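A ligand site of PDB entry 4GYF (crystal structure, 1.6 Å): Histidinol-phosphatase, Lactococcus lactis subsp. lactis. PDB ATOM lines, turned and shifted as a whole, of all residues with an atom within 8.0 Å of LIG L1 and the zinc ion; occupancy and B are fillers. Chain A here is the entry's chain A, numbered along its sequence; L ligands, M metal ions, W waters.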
ATOM      1  N   SER A   2     -10.085 -15.207   1.098  1.00  0.00           N
ATOM      2  CA  SER A   2     -10.364 -16.636   1.217  1.00  0.00           C
ATOM      3  C   SER A   2      -9.077 -17.446   1.082  1.00  0.00           C
ATOM      4  O   SER A   2      -8.148 -17.054   0.363  1.00  0.00           O
ATOM      5  CB  SER A   2     -11.378 -17.072   0.154  1.00  0.00           C
ATOM      6  OG  SER A   2     -10.901 -16.788  -1.148  1.00  0.00           O
ATOM      7  N   LEU A   3      -9.008 -18.569   1.794  1.00  0.00           N
ATOM      8  CA  LEU A   3      -7.849 -19.460   1.691  1.00  0.00           C
ATOM      9  C   LEU A   3      -8.143 -20.533   0.660  1.00  0.00           C
ATOM     10  O   LEU A   3      -9.307 -20.958   0.504  1.00  0.00           O
ATOM     11  CB  LEU A   3      -7.585 -20.143   3.038  1.00  0.00           C
ATOM     12  CG  LEU A   3      -7.301 -19.229   4.234  1.00  0.00           C
ATOM     13  CD1 LEU A   3      -7.212 -20.071   5.510  1.00  0.00           C
ATOM     14  CD2 LEU A   3      -6.041 -18.422   4.013  1.00  0.00           C
ATOM     15  N   LYS A   4      -7.120 -20.974  -0.062  1.00  0.00           N
ATOM     16  CA  LYS A   4      -7.284 -22.091  -0.986  1.00  0.00           C
ATOM     17  C   LYS A   4      -7.802 -23.311  -0.226  1.00  0.00           C
ATOM     18  O   LYS A   4      -7.397 -23.560   0.914  1.00  0.00           O
ATOM     19  CB  LYS A   4      -5.962 -22.436  -1.679  1.00  0.00           C
ATOM     20  CG  LYS A   4      -6.073 -23.553  -2.714  1.00  0.00           C
ATOM     21  CD  LYS A   4      -4.706 -23.888  -3.302  1.00  0.00           C
ATOM     22  CE  LYS A   4      -4.170 -22.748  -4.149  1.00  0.00           C
ATOM     23  NZ  LYS A   4      -4.908 -22.631  -5.434  1.00  0.00           N
ATOM     24  N   LYS A   5      -8.722 -24.047  -0.838  1.00  0.00           N
ATOM     25  CA  LYS A   5      -9.243 -25.255  -0.222  1.00  0.00           C
ATOM     26  C   LYS A   5      -8.275 -26.393  -0.522  1.00  0.00           C
ATOM     27  O   LYS A   5      -8.113 -26.784  -1.687  1.00  0.00           O
ATOM     28  CB  LYS A   5     -10.633 -25.588  -0.782  1.00  0.00           C
ATOM     29  CG  LYS A   5     -11.695 -24.558  -0.403  1.00  0.00           C
ATOM     30  CD  LYS A   5     -12.980 -24.827  -1.169  1.00  0.00           C
ATOM     31  CE  LYS A   5     -12.851 -24.456  -2.646  1.00  0.00           C
ATOM     32  NZ  LYS A   5     -13.878 -25.144  -3.483  1.00  0.00           N
ATOM     33  N   LEU A   6      -7.624 -26.901   0.521  1.00  0.00           N
ATOM     34  CA  LEU A   6      -6.585 -27.916   0.325  1.00  0.00           C
ATOM     35  C   LEU A   6      -6.420 -28.856   1.515  1.00  0.00           C
ATOM     36  O   LEU A   6      -6.963 -28.608   2.585  1.00  0.00           O
ATOM     37  CB  LEU A   6      -5.247 -27.242  -0.028  1.00  0.00           C
ATOM     38  CG  LEU A   6      -4.654 -26.194   0.916  1.00  0.00           C
ATOM     39  CD1 LEU A   6      -4.074 -26.824   2.197  1.00  0.00           C
ATOM     40  CD2 LEU A   6      -3.555 -25.391   0.223  1.00  0.00           C
ATOM     41  N   ALA A  29     -11.621 -35.766  -1.667  1.00  0.00           N
ATOM     42  CA  ALA A  29     -11.208 -34.375  -1.811  1.00  0.00           C
ATOM     43  C   ALA A  29     -12.080 -33.656  -2.851  1.00  0.00           C
ATOM     44  O   ALA A  29     -12.552 -32.532  -2.612  1.00  0.00           O
ATOM     45  CB  ALA A  29      -9.713 -34.311  -2.178  1.00  0.00           C
ATOM     46  N   ALA A  31     -15.102 -34.526  -3.855  1.00  0.00           N
ATOM     47  CA  ALA A  31     -16.462 -34.433  -3.324  1.00  0.00           C
ATOM     48  C   ALA A  31     -16.638 -33.241  -2.389  1.00  0.00           C
ATOM     49  O   ALA A  31     -17.699 -32.589  -2.395  1.00  0.00           O
ATOM     50  CB  ALA A  31     -16.842 -35.732  -2.614  1.00  0.00           C
ATOM     51  N   HIS A  32     -15.613 -32.939  -1.607  1.00  0.00           N
ATOM     52  CA  HIS A  32     -15.680 -31.791  -0.714  1.00  0.00           C
ATOM     53  C   HIS A  32     -15.422 -30.465  -1.428  1.00  0.00           C
ATOM     54  O   HIS A  32     -15.807 -29.413  -0.920  1.00  0.00           O
ATOM     55  CB  HIS A  32     -14.694 -31.934   0.451  1.00  0.00           C
ATOM     56  CG  HIS A  32     -14.881 -30.908   1.530  1.00  0.00           C
ATOM     57  ND1 HIS A  32     -15.920 -30.956   2.429  1.00  0.00           N
ATOM     58  CD2 HIS A  32     -14.173 -29.789   1.826  1.00  0.00           C
ATOM     59  CE1 HIS A  32     -15.847 -29.916   3.239  1.00  0.00           C
ATOM     60  NE2 HIS A  32     -14.795 -29.194   2.898  1.00  0.00           N
ATOM     61  N   GLY A  33     -14.754 -30.527  -2.582  1.00  0.00           N
ATOM     62  CA  GLY A  33     -14.473 -29.325  -3.347  1.00  0.00           C
ATOM     63  C   GLY A  33     -13.081 -28.754  -3.131  1.00  0.00           C
ATOM     64  O   GLY A  33     -12.853 -27.561  -3.351  1.00  0.00           O
ATOM     65  N   LEU A  34     -12.150 -29.599  -2.702  1.00  0.00           N
ATOM     66  CA  LEU A  34     -10.772 -29.163  -2.556  1.00  0.00           C
ATOM     67  C   LEU A  34     -10.159 -28.863  -3.928  1.00  0.00           C
ATOM     68  O   LEU A  34     -10.473 -29.534  -4.928  1.00  0.00           O
ATOM     69  CB  LEU A  34      -9.922 -30.211  -1.819  1.00  0.00           C
ATOM     70  CG  LEU A  34     -10.276 -30.542  -0.380  1.00  0.00           C
ATOM     71  CD1 LEU A  34      -9.168 -31.369   0.279  1.00  0.00           C
ATOM     72  CD2 LEU A  34     -10.563 -29.292   0.444  1.00  0.00           C
ATOM     73  N   GLU A  35      -9.311 -27.847  -3.973  1.00  0.00           N
ATOM     74  CA  GLU A  35      -8.648 -27.410  -5.204  1.00  0.00           C
ATOM     75  C   GLU A  35      -7.278 -28.080  -5.386  1.00  0.00           C
ATOM     76  O   GLU A  35      -6.793 -28.240  -6.511  1.00  0.00           O
ATOM     77  CB  GLU A  35      -8.469 -25.886  -5.180  1.00  0.00           C
ATOM     78  CG  GLU A  35      -9.753 -25.104  -4.882  1.00  0.00           C
ATOM     79  CD  GLU A  35      -9.495 -23.625  -4.586  1.00  0.00           C
ATOM     80  OE1 GLU A  35      -9.051 -22.899  -5.514  1.00  0.00           O
ATOM     81  OE2 GLU A  35      -9.729 -23.182  -3.442  1.00  0.00           O
ATOM     82  N   TRP A 236     -14.150 -32.650   8.442  1.00  0.00           N
ATOM     83  CA  TRP A 236     -14.133 -31.345   7.793  1.00  0.00           C
ATOM     84  C   TRP A 236     -14.375 -30.198   8.770  1.00  0.00           C
ATOM     85  O   TRP A 236     -13.868 -29.102   8.562  1.00  0.00           O
ATOM     86  CB  TRP A 236     -15.158 -31.312   6.648  1.00  0.00           C
ATOM     87  CG  TRP A 236     -14.801 -32.251   5.515  1.00  0.00           C
ATOM     88  CD1 TRP A 236     -15.508 -33.342   5.098  1.00  0.00           C
ATOM     89  CD2 TRP A 236     -13.644 -32.175   4.689  1.00  0.00           C
ATOM     90  NE1 TRP A 236     -14.849 -33.948   4.045  1.00  0.00           N
ATOM     91  CE2 TRP A 236     -13.704 -33.243   3.775  1.00  0.00           C
ATOM     92  CE3 TRP A 236     -12.553 -31.295   4.612  1.00  0.00           C
ATOM     93  CZ2 TRP A 236     -12.720 -33.471   2.810  1.00  0.00           C
ATOM     94  CZ3 TRP A 236     -11.589 -31.515   3.654  1.00  0.00           C
ATOM     95  CH2 TRP A 236     -11.677 -32.586   2.764  1.00  0.00           C
ATOM     96  N   LEU A 237     -15.156 -30.444   9.820  1.00  0.00           N
ATOM     97  CA  LEU A 237     -15.392 -29.423  10.835  1.00  0.00           C
ATOM     98  C   LEU A 237     -14.067 -28.957  11.447  1.00  0.00           C
ATOM     99  O   LEU A 237     -13.851 -27.772  11.678  1.00  0.00           O
ATOM    100  CB  LEU A 237     -16.337 -29.940  11.928  1.00  0.00           C
ATOM    101  CG  LEU A 237     -16.542 -29.014  13.136  1.00  0.00           C
ATOM    102  CD1 LEU A 237     -17.107 -27.684  12.684  1.00  0.00           C
ATOM    103  CD2 LEU A 237     -17.438 -29.647  14.186  1.00  0.00           C
ATOM    104  N   ILE A 239     -11.059 -29.108  10.014  1.00  0.00           N
ATOM    105  CA  ILE A 239     -10.418 -28.306   8.975  1.00  0.00           C
ATOM    106  C   ILE A 239     -10.999 -26.894   8.943  1.00  0.00           C
ATOM    107  O   ILE A 239     -10.266 -25.915   8.857  1.00  0.00           O
ATOM    108  CB  ILE A 239     -10.533 -28.986   7.587  1.00  0.00           C
ATOM    109  CG1 ILE A 239      -9.573 -30.159   7.499  1.00  0.00           C
ATOM    110  CG2 ILE A 239     -10.201 -28.014   6.476  1.00  0.00           C
ATOM    111  CD1 ILE A 239      -8.110 -29.707   7.397  1.00  0.00           C
ATOM    112  N   HIS A 240     -12.327 -26.779   9.018  1.00  0.00           N
ATOM    113  CA  HIS A 240     -12.952 -25.448   8.987  1.00  0.00           C
ATOM    114  C   HIS A 240     -12.572 -24.607  10.197  1.00  0.00           C
ATOM    115  O   HIS A 240     -12.319 -23.403  10.067  1.00  0.00           O
ATOM    116  CB  HIS A 240     -14.460 -25.599   8.823  1.00  0.00           C
ATOM    117  CG  HIS A 240     -14.842 -26.236   7.523  1.00  0.00           C
ATOM    118  ND1 HIS A 240     -15.990 -26.976   7.364  1.00  0.00           N
ATOM    119  CD2 HIS A 240     -14.206 -26.262   6.335  1.00  0.00           C
ATOM    120  CE1 HIS A 240     -16.045 -27.434   6.119  1.00  0.00           C
ATOM    121  NE2 HIS A 240     -14.971 -27.005   5.470  1.00  0.00           N
ATOM    122  N   ARG A 243      -9.043 -23.303   9.531  1.00  0.00           N
ATOM    123  CA  ARG A 243      -9.064 -22.220   8.547  1.00  0.00           C
ATOM    124  C   ARG A 243      -9.498 -20.899   9.179  1.00  0.00           C
ATOM    125  O   ARG A 243      -8.940 -19.842   8.885  1.00  0.00           O
ATOM    126  CB  ARG A 243      -9.958 -22.582   7.345  1.00  0.00           C
ATOM    127  CG  ARG A 243      -9.418 -23.795   6.564  1.00  0.00           C
ATOM    128  CD  ARG A 243     -10.461 -24.386   5.590  1.00  0.00           C
ATOM    129  NE  ARG A 243     -10.886 -23.390   4.615  1.00  0.00           N
ATOM    130  CZ  ARG A 243     -10.201 -23.084   3.508  1.00  0.00           C
ATOM    131  NH1 ARG A 243      -9.065 -23.715   3.214  1.00  0.00           N
ATOM    132  NH2 ARG A 243     -10.657 -22.143   2.685  1.00  0.00           N
ATOM    133  N   LYS A 247      -7.098 -17.403   9.426  1.00  0.00           N
ATOM    134  CA  LYS A 247      -7.532 -16.082   8.983  1.00  0.00           C
ATOM    135  C   LYS A 247      -7.564 -15.068  10.127  1.00  0.00           C
ATOM    136  O   LYS A 247      -7.138 -13.917   9.959  1.00  0.00           O
ATOM    137  CB  LYS A 247      -8.915 -16.178   8.318  1.00  0.00           C
ATOM    138  CG  LYS A 247      -8.848 -16.701   6.897  1.00  0.00           C
ATOM    139  CD  LYS A 247     -10.229 -16.783   6.265  1.00  0.00           C
ATOM    140  CE  LYS A 247     -11.084 -17.855   6.912  1.00  0.00           C
ATOM    141  NZ  LYS A 247     -12.334 -18.104   6.136  1.00  0.00           N
HETATM  142  N1  LIG L   1     -15.723 -20.434   0.771  1.00  0.00           N
HETATM  143  C1  LIG L   1     -15.264 -21.720   1.307  1.00  0.00           C
HETATM  144  C2  LIG L   1     -16.002 -22.886   0.636  1.00  0.00           C
HETATM  145  C3  LIG L   1     -15.760 -24.287   1.149  1.00  0.00           C
HETATM  146  N2  LIG L   1     -15.952 -25.414   0.424  1.00  0.00           N
HETATM  147  C4  LIG L   1     -15.288 -24.675   2.402  1.00  0.00           C
HETATM  148  C5  LIG L   1     -15.617 -26.475   1.185  1.00  0.00           C
HETATM  149  N3  LIG L   1     -15.219 -26.030   2.394  1.00  0.00           N
HETATM  150  C6  LIG L   1     -13.782 -21.825   0.959  1.00  0.00           C
HETATM  151  O1  LIG L   1     -13.410 -21.627  -0.192  1.00  0.00           O
HETATM  152 CL1  LG2 L   2     -12.136 -27.045   3.388  1.00  0.00          CL
HETATM  153 ZN    ZN M   1     -14.300 -27.364   3.579  1.00  0.00          ZN
HETATM  154  O   HOH W   1     -15.263 -20.459  -2.401  1.00  0.00           O
HETATM  155  O   HOH W   2     -11.291 -20.527  -1.098  1.00  0.00           O
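NH2 of Arg 243 is in hydrogen-bond range of O of Leu 3.
The backbone carbonyl oxygen of Gly 33 is in hydrogen-bond range of the side-chain amino group of Lys 5.
The backbone carbonyl oxygen (O) of Lys 5 lies within hydrogen-bond range of the backbone NH (N) of Glu 35, at 2.8 Å.
The backbone carbonyl oxygen (O) of Trp 236 lies close to a ring nitrogen (ND1) of His 240.
The backbone carbonyl oxygen (O) of Lys 4 is in hydrogen-bond range of the guanidinium group (NH1) of Arg 243, at 2.8 Å.
Merely in contact with LIG L1: Lys 5 (3.4 Å) and Arg 243 (3.6 Å).
Hydrophobic or aromatic side chains that line LIG L1: His 32.
Within 4 Å of LIG L1: Lys 5, His 32, His 240 and Arg 243.
The nearest printed residue that does not touch LIG L1 is Leu 3 (4.2 Å).
Two residues have an atom within 4 Å of the zinc ion: His 32 and His 240.
Along chain A the residues within 4 Å of the zinc ion span positions 32 to 240.
The nearest printed residue that does not touch the zinc ion is Trp 236 (4.4 Å).
The zinc ion is bound by a nitrogen (N3) of LIG L1, a ring nitrogen (NE2) of His 32, a ring nitrogen (NE2) of His 240 and a chlorine (CL1) of LG2 L2.
Water W2 lies within hydrogen-bond range of an oxygen (O1) of LIG L1 (2.6 Å) and the backbone carbonyl oxygen of Leu 3 (2.6 Å).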
